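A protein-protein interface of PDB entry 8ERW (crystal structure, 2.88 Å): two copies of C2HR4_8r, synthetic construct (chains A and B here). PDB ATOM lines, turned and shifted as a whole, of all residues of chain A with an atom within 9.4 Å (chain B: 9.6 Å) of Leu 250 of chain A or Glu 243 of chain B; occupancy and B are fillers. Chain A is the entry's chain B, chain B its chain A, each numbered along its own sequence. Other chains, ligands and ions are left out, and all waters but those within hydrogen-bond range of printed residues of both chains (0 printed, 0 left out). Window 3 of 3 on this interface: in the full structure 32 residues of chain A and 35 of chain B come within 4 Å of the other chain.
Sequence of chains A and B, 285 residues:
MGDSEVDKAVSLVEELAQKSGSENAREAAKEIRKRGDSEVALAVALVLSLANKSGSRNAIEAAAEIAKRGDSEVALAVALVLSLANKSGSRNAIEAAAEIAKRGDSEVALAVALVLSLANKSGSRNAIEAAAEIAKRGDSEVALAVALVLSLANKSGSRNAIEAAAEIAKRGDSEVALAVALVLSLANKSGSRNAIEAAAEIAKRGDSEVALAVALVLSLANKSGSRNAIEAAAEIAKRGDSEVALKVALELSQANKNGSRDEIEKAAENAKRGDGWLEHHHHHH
The backbone NH (N) of Glu 243 of chain B lies close to the side-chain carboxylate (OD1) of Asp 241 of chain B.
Among the printed residues, pairs that only touch across the chains: Leu 216 of chain A with Leu 216 of chain B, Leu 246 of chain A with Leu 216 of chain B, Leu 216 of chain A with Leu 246 of chain B, Ala 213 of chain A with Leu 216 of chain B, Leu 216 of chain A with Ala 213 of chain B, Leu 246 of chain A with Leu 246 of chain B and Leu 250 of chain A with Glu 243 of chain B.
Leu 250 of chain A touches just one residue of chain B: Glu 243.
Of chain A, only Leu 250 (3.9 Å) comes within 4 Å of Glu 243 of chain B.
No residue of chain B comes within 4 Å of Glu 251 of chain A.
No residue of chain B comes within 4 Å of Ser 253 of chain A.
No residue of chain A comes within 4 Å of Val 244 of chain B.
Printed residues of chain B within 4 Å of Leu 216 of chain A: Ala 213 (3.7 Å), Leu 216 (3.1 Å) and Leu 246 (3.4 Å).
Printed residues of chain A within 4 Å of Ala 213 of chain B: Leu 216.
Of the printed residues of chain B, Leu 246 of chain A touches Leu 216 and Leu 246.
Glu 209 of chain B touches none of the printed residues of chain A.
Val 244 of chain A touches none of the printed residues of chain B.
The nearest residue of chain A that does not touch Glu 243 of chain B is Gln 254 of chain A (4.8 Å).
The nearest printed residue of chain B that does not touch Leu 246 of chain A is Leu 250 of chain B (4.3 Å).
Of the 23 printed residues of chain A, 4 touch a printed residue of chain B.
Hydrophobic or aromatic side chains of chain A within 4 Å of the printed part of chain B: Leu 216, Leu 246 and Leu 250.
Among the printed residues, 7 pairs touch across the chains.
Ala 213 of chain A touches Leu 216 of chain B, and with the chains exchanged Leu 216 of chain A touches Ala 213 of chain B.
Leu 216 of chain A touches its own counterpart, Leu 216 of chain B.
Leu 246 of chain A touches its own counterpart, Leu 246 of chain B.
Leu 250 of chain A touches Glu 243 of chain B, but with the chains exchanged Glu 243 of chain A does not touch Leu 250 of chain B (4.02 Å).
Of the 7 pairs that touch across the chains among the printed residues, 6 have their exchanged pair printed and touching as well.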
ATOM      1  N   ALA A 213      24.828 -32.474   5.222  1.00  0.00           N
ATOM      2  CA  ALA A 213      25.877 -33.055   6.052  1.00  0.00           C
ATOM      3  C   ALA A 213      27.217 -33.018   5.328  1.00  0.00           C
ATOM      4  O   ALA A 213      28.255 -32.728   5.935  1.00  0.00           O
ATOM      5  CB  ALA A 213      25.512 -34.488   6.439  1.00  0.00           C
ATOM      6  N   LEU A 216      28.461 -29.315   4.927  1.00  0.00           N
ATOM      7  CA  LEU A 216      29.216 -28.913   6.106  1.00  0.00           C
ATOM      8  C   LEU A 216      30.657 -29.392   6.020  1.00  0.00           C
ATOM      9  O   LEU A 216      31.604 -28.604   6.135  1.00  0.00           O
ATOM     10  CB  LEU A 216      28.572 -29.488   7.359  1.00  0.00           C
ATOM     11  CG  LEU A 216      27.300 -28.861   7.890  1.00  0.00           C
ATOM     12  CD1 LEU A 216      26.803 -29.806   8.965  1.00  0.00           C
ATOM     13  CD2 LEU A 216      27.542 -27.490   8.433  1.00  0.00           C
ATOM     14  N   VAL A 217      30.831 -30.705   5.860  1.00  0.00           N
ATOM     15  CA  VAL A 217      32.166 -31.291   5.839  1.00  0.00           C
ATOM     16  C   VAL A 217      33.051 -30.547   4.853  1.00  0.00           C
ATOM     17  O   VAL A 217      34.134 -30.061   5.205  1.00  0.00           O
ATOM     18  CB  VAL A 217      32.073 -32.792   5.499  1.00  0.00           C
ATOM     19  CG1 VAL A 217      33.447 -33.341   5.187  1.00  0.00           C
ATOM     20  CG2 VAL A 217      31.433 -33.552   6.650  1.00  0.00           C
ATOM     21  N   LEU A 220      33.773 -27.134   6.001  1.00  0.00           N
ATOM     22  CA  LEU A 220      34.708 -27.105   7.118  1.00  0.00           C
ATOM     23  C   LEU A 220      36.109 -27.513   6.689  1.00  0.00           C
ATOM     24  O   LEU A 220      37.093 -27.018   7.250  1.00  0.00           O
ATOM     25  CB  LEU A 220      34.207 -28.008   8.244  1.00  0.00           C
ATOM     26  CG  LEU A 220      33.118 -27.389   9.121  1.00  0.00           C
ATOM     27  CD1 LEU A 220      32.571 -28.401  10.109  1.00  0.00           C
ATOM     28  CD2 LEU A 220      33.657 -26.170   9.858  1.00  0.00           C
ATOM     29  N   ILE A 236      34.290 -38.952   2.181  1.00  0.00           N
ATOM     30  CA  ILE A 236      33.012 -39.010   2.883  1.00  0.00           C
ATOM     31  C   ILE A 236      31.863 -38.801   1.908  1.00  0.00           C
ATOM     32  O   ILE A 236      30.859 -39.524   1.935  1.00  0.00           O
ATOM     33  CB  ILE A 236      32.978 -37.965   4.012  1.00  0.00           C
ATOM     34  CG1 ILE A 236      34.066 -38.265   5.038  1.00  0.00           C
ATOM     35  CG2 ILE A 236      31.617 -37.945   4.669  1.00  0.00           C
ATOM     36  CD1 ILE A 236      34.344 -37.106   5.957  1.00  0.00           C
ATOM     37  N   SER A 242      25.237 -40.075   5.735  1.00  0.00           N
ATOM     38  CA  SER A 242      24.838 -38.858   6.435  1.00  0.00           C
ATOM     39  C   SER A 242      25.434 -38.792   7.836  1.00  0.00           C
ATOM     40  O   SER A 242      26.006 -37.770   8.233  1.00  0.00           O
ATOM     41  CB  SER A 242      23.311 -38.788   6.491  1.00  0.00           C
ATOM     42  OG  SER A 242      22.876 -37.743   7.338  1.00  0.00           O
ATOM     43  N   GLU A 243      25.311 -39.879   8.601  1.00  0.00           N
ATOM     44  CA  GLU A 243      25.782 -39.860   9.982  1.00  0.00           C
ATOM     45  C   GLU A 243      27.288 -39.670  10.062  1.00  0.00           C
ATOM     46  O   GLU A 243      27.784 -39.022  10.992  1.00  0.00           O
ATOM     47  CB  GLU A 243      25.381 -41.154  10.692  1.00  0.00           C
ATOM     48  N   VAL A 244      28.032 -40.224   9.105  1.00  0.00           N
ATOM     49  CA  VAL A 244      29.486 -40.141   9.170  1.00  0.00           C
ATOM     50  C   VAL A 244      29.949 -38.722   8.881  1.00  0.00           C
ATOM     51  O   VAL A 244      30.880 -38.215   9.519  1.00  0.00           O
ATOM     52  CB  VAL A 244      30.124 -41.154   8.202  1.00  0.00           C
ATOM     53  CG1 VAL A 244      31.632 -41.141   8.361  1.00  0.00           C
ATOM     54  CG2 VAL A 244      29.565 -42.542   8.446  1.00  0.00           C
ATOM     55  N   ALA A 245      29.319 -38.061   7.908  1.00  0.00           N
ATOM     56  CA  ALA A 245      29.661 -36.671   7.629  1.00  0.00           C
ATOM     57  C   ALA A 245      29.446 -35.801   8.861  1.00  0.00           C
ATOM     58  O   ALA A 245      30.286 -34.954   9.188  1.00  0.00           O
ATOM     59  CB  ALA A 245      28.834 -36.153   6.452  1.00  0.00           C
ATOM     60  N   LEU A 246      28.328 -36.004   9.563  1.00  0.00           N
ATOM     61  CA  LEU A 246      28.065 -35.219  10.765  1.00  0.00           C
ATOM     62  C   LEU A 246      29.067 -35.543  11.866  1.00  0.00           C
ATOM     63  O   LEU A 246      29.506 -34.648  12.596  1.00  0.00           O
ATOM     64  CB  LEU A 246      26.639 -35.469  11.253  1.00  0.00           C
ATOM     65  CG  LEU A 246      25.548 -34.941  10.322  1.00  0.00           C
ATOM     66  CD1 LEU A 246      24.170 -35.318  10.820  1.00  0.00           C
ATOM     67  CD2 LEU A 246      25.677 -33.430  10.188  1.00  0.00           C
ATOM     68  N   LYS A 247      29.433 -36.820  12.005  1.00  0.00           N
ATOM     69  CA  LYS A 247      30.453 -37.190  12.979  1.00  0.00           C
ATOM     70  C   LYS A 247      31.768 -36.484  12.676  1.00  0.00           C
ATOM     71  O   LYS A 247      32.408 -35.919  13.572  1.00  0.00           O
ATOM     72  CB  LYS A 247      30.641 -38.706  12.988  1.00  0.00           C
ATOM     73  N   VAL A 248      32.187 -36.504  11.408  1.00  0.00           N
ATOM     74  CA  VAL A 248      33.393 -35.784  11.016  1.00  0.00           C
ATOM     75  C   VAL A 248      33.175 -34.283  11.132  1.00  0.00           C
ATOM     76  O   VAL A 248      34.071 -33.544  11.557  1.00  0.00           O
ATOM     77  CB  VAL A 248      33.811 -36.177   9.587  1.00  0.00           C
ATOM     78  CG1 VAL A 248      34.917 -35.257   9.091  1.00  0.00           C
ATOM     79  CG2 VAL A 248      34.255 -37.626   9.543  1.00  0.00           C
ATOM     80  N   ALA A 249      31.990 -33.804  10.745  1.00  0.00           N
ATOM     81  CA  ALA A 249      31.678 -32.387  10.898  1.00  0.00           C
ATOM     82  C   ALA A 249      31.925 -31.929  12.329  1.00  0.00           C
ATOM     83  O   ALA A 249      32.506 -30.862  12.559  1.00  0.00           O
ATOM     84  CB  ALA A 249      30.229 -32.123  10.489  1.00  0.00           C
ATOM     85  N   LEU A 250      31.488 -32.728  13.306  1.00  0.00           N
ATOM     86  CA  LEU A 250      31.822 -32.454  14.699  1.00  0.00           C
ATOM     87  C   LEU A 250      33.332 -32.462  14.906  1.00  0.00           C
ATOM     88  O   LEU A 250      33.916 -31.489  15.399  1.00  0.00           O
ATOM     89  CB  LEU A 250      31.165 -33.492  15.609  1.00  0.00           C
ATOM     90  CG  LEU A 250      29.863 -33.109  16.303  1.00  0.00           C
ATOM     91  CD1 LEU A 250      29.350 -34.294  17.117  1.00  0.00           C
ATOM     92  CD2 LEU A 250      30.058 -31.886  17.182  1.00  0.00           C
ATOM     93  N   GLU A 251      33.980 -33.571  14.547  1.00  0.00           N
ATOM     94  CA  GLU A 251      35.420 -33.681  14.746  1.00  0.00           C
ATOM     95  C   GLU A 251      36.163 -32.590  13.990  1.00  0.00           C
ATOM     96  O   GLU A 251      37.167 -32.058  14.478  1.00  0.00           O
ATOM     97  CB  GLU A 251      35.906 -35.064  14.309  1.00  0.00           C
ATOM     98  N   LEU A 252      35.687 -32.240  12.794  1.00  0.00           N
ATOM     99  CA  LEU A 252      36.365 -31.218  12.007  1.00  0.00           C
ATOM    100  C   LEU A 252      36.067 -29.816  12.516  1.00  0.00           C
ATOM    101  O   LEU A 252      36.931 -28.936  12.437  1.00  0.00           O
ATOM    102  CB  LEU A 252      35.958 -31.332  10.540  1.00  0.00           C
ATOM    103  CG  LEU A 252      37.060 -31.695   9.542  1.00  0.00           C
ATOM    104  CD1 LEU A 252      36.509 -31.659   8.124  1.00  0.00           C
ATOM    105  CD2 LEU A 252      38.249 -30.764   9.682  1.00  0.00           C
ATOM    106  N   SER A 253      34.861 -29.591  13.041  1.00  0.00           N
ATOM    107  CA  SER A 253      34.485 -28.256  13.492  1.00  0.00           C
ATOM    108  C   SER A 253      35.336 -27.817  14.678  1.00  0.00           C
ATOM    109  O   SER A 253      35.851 -26.694  14.705  1.00  0.00           O
ATOM    110  CB  SER A 253      33.000 -28.229  13.861  1.00  0.00           C
ATOM    111  N   GLN A 254      35.493 -28.695  15.671  1.00  0.00           N
ATOM    112  CA  GLN A 254      36.171 -28.306  16.903  1.00  0.00           C
ATOM    113  C   GLN A 254      37.648 -28.021  16.664  1.00  0.00           C
ATOM    114  O   GLN A 254      38.210 -27.097  17.264  1.00  0.00           O
ATOM    115  CB  GLN A 254      35.982 -29.397  17.956  1.00  0.00           C
ATOM    116  CG  GLN A 254      34.515 -29.736  18.198  1.00  0.00           C
ATOM    117  CD  GLN A 254      34.316 -30.799  19.259  1.00  0.00           C
ATOM    118  OE1 GLN A 254      35.082 -31.759  19.346  1.00  0.00           O
ATOM    119  NE2 GLN A 254      33.283 -30.629  20.077  1.00  0.00           N
ATOM    120  N   ALA A 255      38.295 -28.793  15.787  1.00  0.00           N
ATOM    121  CA  ALA A 255      39.680 -28.492  15.438  1.00  0.00           C
ATOM    122  C   ALA A 255      39.789 -27.124  14.777  1.00  0.00           C
ATOM    123  O   ALA A 255      40.755 -26.386  15.009  1.00  0.00           O
ATOM    124  CB  ALA A 255      40.243 -29.575  14.518  1.00  0.00           C
ATOM    125  N   ASN A 256      38.810 -26.770  13.940  1.00  0.00           N
ATOM    126  CA  ASN A 256      38.804 -25.442  13.335  1.00  0.00           C
ATOM    127  C   ASN A 256      38.787 -24.354  14.403  1.00  0.00           C
ATOM    128  O   ASN A 256      39.503 -23.352  14.290  1.00  0.00           O
ATOM    129  CB  ASN A 256      37.602 -25.291  12.402  1.00  0.00           C
ATOM    130  CG  ASN A 256      37.933 -25.624  10.959  1.00  0.00           C
ATOM    131  OD1 ASN A 256      38.610 -26.612  10.672  1.00  0.00           O
ATOM    132  ND2 ASN A 256      37.462 -24.787  10.038  1.00  0.00           N
ATOM    133  N   LYS A 257      37.979 -24.535  15.445  1.00  0.00           N
ATOM    134  CA  LYS A 257      37.883 -23.557  16.524  1.00  0.00           C
ATOM    135  C   LYS A 257      39.229 -23.380  17.220  1.00  0.00           C
ATOM    136  O   LYS A 257      39.592 -22.273  17.615  1.00  0.00           O
ATOM    137  CB  LYS A 257      36.821 -23.981  17.542  1.00  0.00           C
ATOM    138  N   GLU A 263      46.154 -30.680  14.281  1.00  0.00           N
ATOM    139  CA  GLU A 263      44.987 -31.501  14.578  1.00  0.00           C
ATOM    140  C   GLU A 263      44.047 -31.674  13.393  1.00  0.00           C
ATOM    141  O   GLU A 263      43.405 -32.724  13.282  1.00  0.00           O
ATOM    142  CB  GLU A 263      44.214 -30.892  15.752  1.00  0.00           C
ATOM    143  CG  GLU A 263      43.084 -31.753  16.271  1.00  0.00           C
ATOM    144  CD  GLU A 263      42.850 -31.560  17.756  1.00  0.00           C
ATOM    145  OE1 GLU A 263      43.841 -31.515  18.515  1.00  0.00           O
ATOM    146  OE2 GLU A 263      41.674 -31.448  18.164  1.00  0.00           O
ATOM    147  N   ALA A 267      41.905 -35.327  12.472  1.00  0.00           N
ATOM    148  CA  ALA A 267      40.501 -35.605  12.188  1.00  0.00           C
ATOM    149  C   ALA A 267      40.287 -35.967  10.726  1.00  0.00           C
ATOM    150  O   ALA A 267      39.390 -36.755  10.407  1.00  0.00           O
ATOM    151  CB  ALA A 267      39.641 -34.398  12.568  1.00  0.00           C
ATOM    152  N   ASP B 207      27.088 -16.342   9.942  1.00  0.00           N
ATOM    153  CA  ASP B 207      28.055 -17.427  10.057  1.00  0.00           C
ATOM    154  C   ASP B 207      27.585 -18.614   9.225  1.00  0.00           C
ATOM    155  O   ASP B 207      26.503 -19.158   9.469  1.00  0.00           O
ATOM    156  CB  ASP B 207      28.242 -17.841  11.517  1.00  0.00           C
ATOM    157  CG  ASP B 207      29.376 -18.834  11.704  1.00  0.00           C
ATOM    158  OD1 ASP B 207      29.808 -19.452  10.707  1.00  0.00           O
ATOM    159  OD2 ASP B 207      29.831 -19.004  12.855  1.00  0.00           O
ATOM    160  N   GLU B 209      28.851 -21.729   9.012  1.00  0.00           N
ATOM    161  CA  GLU B 209      28.813 -22.991   9.742  1.00  0.00           C
ATOM    162  C   GLU B 209      27.591 -23.066  10.649  1.00  0.00           C
ATOM    163  O   GLU B 209      26.990 -24.135  10.807  1.00  0.00           O
ATOM    164  CB  GLU B 209      30.097 -23.167  10.556  1.00  0.00           C
ATOM    165  N   VAL B 210      27.203 -21.937  11.247  1.00  0.00           N
ATOM    166  CA  VAL B 210      26.042 -21.926  12.132  1.00  0.00           C
ATOM    167  C   VAL B 210      24.765 -22.161  11.332  1.00  0.00           C
ATOM    168  O   VAL B 210      23.944 -23.016  11.679  1.00  0.00           O
ATOM    169  CB  VAL B 210      25.975 -20.600  12.914  1.00  0.00           C
ATOM    170  CG1 VAL B 210      24.779 -20.596  13.864  1.00  0.00           C
ATOM    171  CG2 VAL B 210      27.266 -20.360  13.680  1.00  0.00           C
ATOM    172  N   ALA B 211      24.580 -21.405  10.247  1.00  0.00           N
ATOM    173  CA  ALA B 211      23.363 -21.535   9.453  1.00  0.00           C
ATOM    174  C   ALA B 211      23.188 -22.959   8.937  1.00  0.00           C
ATOM    175  O   ALA B 211      22.107 -23.549   9.060  1.00  0.00           O
ATOM    176  CB  ALA B 211      23.385 -20.542   8.288  1.00  0.00           C
ATOM    177  N   ALA B 213      24.568 -25.912   9.995  1.00  0.00           N
ATOM    178  CA  ALA B 213      24.263 -26.792  11.118  1.00  0.00           C
ATOM    179  C   ALA B 213      22.818 -26.620  11.569  1.00  0.00           C
ATOM    180  O   ALA B 213      22.135 -27.601  11.887  1.00  0.00           O
ATOM    181  CB  ALA B 213      25.222 -26.515  12.277  1.00  0.00           C
ATOM    182  N   VAL B 214      22.333 -25.377  11.585  1.00  0.00           N
ATOM    183  CA  VAL B 214      20.941 -25.125  11.936  1.00  0.00           C
ATOM    184  C   VAL B 214      20.017 -25.596  10.824  1.00  0.00           C
ATOM    185  O   VAL B 214      18.968 -26.198  11.083  1.00  0.00           O
ATOM    186  CB  VAL B 214      20.736 -23.631  12.244  1.00  0.00           C
ATOM    187  CG1 VAL B 214      19.258 -23.328  12.436  1.00  0.00           C
ATOM    188  CG2 VAL B 214      21.534 -23.234  13.468  1.00  0.00           C
ATOM    189  N   LEU B 216      20.398 -28.049   8.882  1.00  0.00           N
ATOM    190  CA  LEU B 216      20.246 -29.475   9.129  1.00  0.00           C
ATOM    191  C   LEU B 216      19.132 -29.742  10.129  1.00  0.00           C
ATOM    192  O   LEU B 216      18.145 -30.425   9.828  1.00  0.00           O
ATOM    193  CB  LEU B 216      21.553 -30.049   9.662  1.00  0.00           C
ATOM    194  CG  LEU B 216      22.740 -30.233   8.735  1.00  0.00           C
ATOM    195  CD1 LEU B 216      23.897 -30.691   9.610  1.00  0.00           C
ATOM    196  CD2 LEU B 216      22.451 -31.226   7.651  1.00  0.00           C
ATOM    197  N   VAL B 217      19.299 -29.222  11.349  1.00  0.00           N
ATOM    198  CA  VAL B 217      18.341 -29.479  12.421  1.00  0.00           C
ATOM    199  C   VAL B 217      16.924 -29.205  11.944  1.00  0.00           C
ATOM    200  O   VAL B 217      16.028 -30.047  12.085  1.00  0.00           O
ATOM    201  CB  VAL B 217      18.695 -28.632  13.656  1.00  0.00           C
ATOM    202  CG1 VAL B 217      17.654 -28.806  14.743  1.00  0.00           C
ATOM    203  CG2 VAL B 217      20.081 -29.007  14.177  1.00  0.00           C
ATOM    204  N   ILE B 236      17.486 -24.156  19.494  1.00  0.00           N
ATOM    205  CA  ILE B 236      18.881 -24.339  19.106  1.00  0.00           C
ATOM    206  C   ILE B 236      19.346 -23.180  18.236  1.00  0.00           C
ATOM    207  O   ILE B 236      20.435 -22.629  18.430  1.00  0.00           O
ATOM    208  CB  ILE B 236      19.059 -25.684  18.380  1.00  0.00           C
ATOM    209  CG1 ILE B 236      18.734 -26.845  19.315  1.00  0.00           C
ATOM    210  CG2 ILE B 236      20.471 -25.811  17.844  1.00  0.00           C
ATOM    211  CD1 ILE B 236      18.666 -28.174  18.606  1.00  0.00           C
ATOM    212  N   ARG B 239      20.203 -20.133  20.246  1.00  0.00           N
ATOM    213  CA  ARG B 239      21.500 -20.256  20.902  1.00  0.00           C
ATOM    214  C   ARG B 239      22.641 -19.987  19.926  1.00  0.00           C
ATOM    215  O   ARG B 239      23.652 -19.378  20.292  1.00  0.00           O
ATOM    216  CB  ARG B 239      21.648 -21.648  21.523  1.00  0.00           C
ATOM    217  CG  ARG B 239      21.276 -21.735  22.998  1.00  0.00           C
ATOM    218  CD  ARG B 239      21.115 -23.193  23.449  1.00  0.00           C
ATOM    219  NE  ARG B 239      22.360 -23.948  23.373  1.00  0.00           N
ATOM    220  CZ  ARG B 239      22.992 -24.475  24.415  1.00  0.00           C
ATOM    221  NH1 ARG B 239      22.499 -24.390  25.642  1.00  0.00           N
ATOM    222  NH2 ARG B 239      24.146 -25.109  24.221  1.00  0.00           N
ATOM    223  N   GLY B 240      22.498 -20.438  18.680  1.00  0.00           N
ATOM    224  CA  GLY B 240      23.534 -20.216  17.694  1.00  0.00           C
ATOM    225  C   GLY B 240      24.806 -20.990  17.922  1.00  0.00           C
ATOM    226  O   GLY B 240      25.864 -20.584  17.434  1.00  0.00           O
ATOM    227  N   ASP B 241      24.735 -22.099  18.654  1.00  0.00           N
ATOM    228  CA  ASP B 241      25.910 -22.906  18.969  1.00  0.00           C
ATOM    229  C   ASP B 241      26.037 -24.008  17.923  1.00  0.00           C
ATOM    230  O   ASP B 241      25.259 -24.968  17.919  1.00  0.00           O
ATOM    231  CB  ASP B 241      25.799 -23.493  20.374  1.00  0.00           C
ATOM    232  CG  ASP B 241      27.131 -23.988  20.905  1.00  0.00           C
ATOM    233  OD1 ASP B 241      28.053 -24.213  20.091  1.00  0.00           O
ATOM    234  OD2 ASP B 241      27.256 -24.154  22.136  1.00  0.00           O
ATOM    235  N   SER B 242      27.029 -23.870  17.039  1.00  0.00           N
ATOM    236  CA  SER B 242      27.189 -24.815  15.940  1.00  0.00           C
ATOM    237  C   SER B 242      27.408 -26.236  16.449  1.00  0.00           C
ATOM    238  O   SER B 242      26.826 -27.188  15.915  1.00  0.00           O
ATOM    239  CB  SER B 242      28.357 -24.380  15.057  1.00  0.00           C
ATOM    240  OG  SER B 242      28.679 -25.379  14.109  1.00  0.00           O
ATOM    241  N   GLU B 243      28.249 -26.402  17.472  1.00  0.00           N
ATOM    242  CA  GLU B 243      28.519 -27.741  17.983  1.00  0.00           C
ATOM    243  C   GLU B 243      27.258 -28.393  18.528  1.00  0.00           C
ATOM    244  O   GLU B 243      27.080 -29.610  18.399  1.00  0.00           O
ATOM    245  CB  GLU B 243      29.595 -27.683  19.069  1.00  0.00           C
ATOM    246  N   VAL B 244      26.367 -27.603  19.127  1.00  0.00           N
ATOM    247  CA  VAL B 244      25.164 -28.168  19.727  1.00  0.00           C
ATOM    248  C   VAL B 244      24.145 -28.532  18.654  1.00  0.00           C
ATOM    249  O   VAL B 244      23.382 -29.491  18.823  1.00  0.00           O
ATOM    250  CB  VAL B 244      24.569 -27.184  20.750  1.00  0.00           C
ATOM    251  CG1 VAL B 244      23.380 -27.817  21.458  1.00  0.00           C
ATOM    252  CG2 VAL B 244      25.633 -26.745  21.748  1.00  0.00           C
ATOM    253  N   ALA B 245      24.107 -27.785  17.550  1.00  0.00           N
ATOM    254  CA  ALA B 245      23.176 -28.103  16.475  1.00  0.00           C
ATOM    255  C   ALA B 245      23.518 -29.439  15.828  1.00  0.00           C
ATOM    256  O   ALA B 245      22.620 -30.221  15.497  1.00  0.00           O
ATOM    257  CB  ALA B 245      23.179 -26.986  15.430  1.00  0.00           C
ATOM    258  N   LEU B 246      24.810 -29.717  15.640  1.00  0.00           N
ATOM    259  CA  LEU B 246      25.208 -30.971  15.007  1.00  0.00           C
ATOM    260  C   LEU B 246      24.943 -32.161  15.923  1.00  0.00           C
ATOM    261  O   LEU B 246      24.579 -33.245  15.455  1.00  0.00           O
ATOM    262  CB  LEU B 246      26.682 -30.917  14.615  1.00  0.00           C
ATOM    263  CG  LEU B 246      27.003 -29.873  13.547  1.00  0.00           C
ATOM    264  CD1 LEU B 246      28.487 -29.798  13.266  1.00  0.00           C
ATOM    265  CD2 LEU B 246      26.227 -30.192  12.272  1.00  0.00           C
ATOM    266  N   LYS B 247      25.136 -31.984  17.232  1.00  0.00           N
ATOM    267  CA  LYS B 247      24.828 -33.057  18.173  1.00  0.00           C
ATOM    268  C   LYS B 247      23.348 -33.418  18.111  1.00  0.00           C
ATOM    269  O   LYS B 247      22.986 -34.596  18.000  1.00  0.00           O
ATOM    270  CB  LYS B 247      25.223 -32.644  19.591  1.00  0.00           C
ATOM    271  N   VAL B 248      22.477 -32.410  18.182  1.00  0.00           N
ATOM    272  CA  VAL B 248      21.046 -32.658  18.056  1.00  0.00           C
ATOM    273  C   VAL B 248      20.715 -33.150  16.654  1.00  0.00           C
ATOM    274  O   VAL B 248      19.841 -34.007  16.474  1.00  0.00           O
ATOM    275  CB  VAL B 248      20.251 -31.388  18.410  1.00  0.00           C
ATOM    276  CG1 VAL B 248      18.799 -31.530  17.975  1.00  0.00           C
ATOM    277  CG2 VAL B 248      20.341 -31.112  19.901  1.00  0.00           C
ATOM    278  N   ALA B 249      21.398 -32.613  15.640  1.00  0.00           N
ATOM    279  CA  ALA B 249      21.200 -33.105  14.281  1.00  0.00           C
ATOM    280  C   ALA B 249      21.463 -34.603  14.203  1.00  0.00           C
ATOM    281  O   ALA B 249      20.697 -35.345  13.574  1.00  0.00           O
ATOM    282  CB  ALA B 249      22.111 -32.351  13.310  1.00  0.00           C
ATOM    283  N   LEU B 250      22.540 -35.067  14.838  1.00  0.00           N
ATOM    284  CA  LEU B 250      22.824 -36.497  14.862  1.00  0.00           C
ATOM    285  C   LEU B 250      21.741 -37.248  15.624  1.00  0.00           C
ATOM    286  O   LEU B 250      21.210 -38.257  15.144  1.00  0.00           O
ATOM    287  CB  LEU B 250      24.193 -36.748  15.492  1.00  0.00           C
ATOM    288  CG  LEU B 250      24.745 -38.164  15.320  1.00  0.00           C
ATOM    289  CD1 LEU B 250      25.023 -38.424  13.847  1.00  0.00           C
ATOM    290  CD2 LEU B 250      25.991 -38.364  16.157  1.00  0.00           C
ATOM    291  N   GLU B 251      21.401 -36.768  16.822  1.00  0.00           N
ATOM    292  CA  GLU B 251      20.327 -37.396  17.583  1.00  0.00           C
ATOM    293  C   GLU B 251      19.015 -37.357  16.811  1.00  0.00           C
ATOM    294  O   GLU B 251      18.232 -38.313  16.854  1.00  0.00           O
ATOM    295  CB  GLU B 251      20.172 -36.711  18.941  1.00  0.00           C
ATOM    296  CG  GLU B 251      21.069 -37.280  20.029  1.00  0.00           C
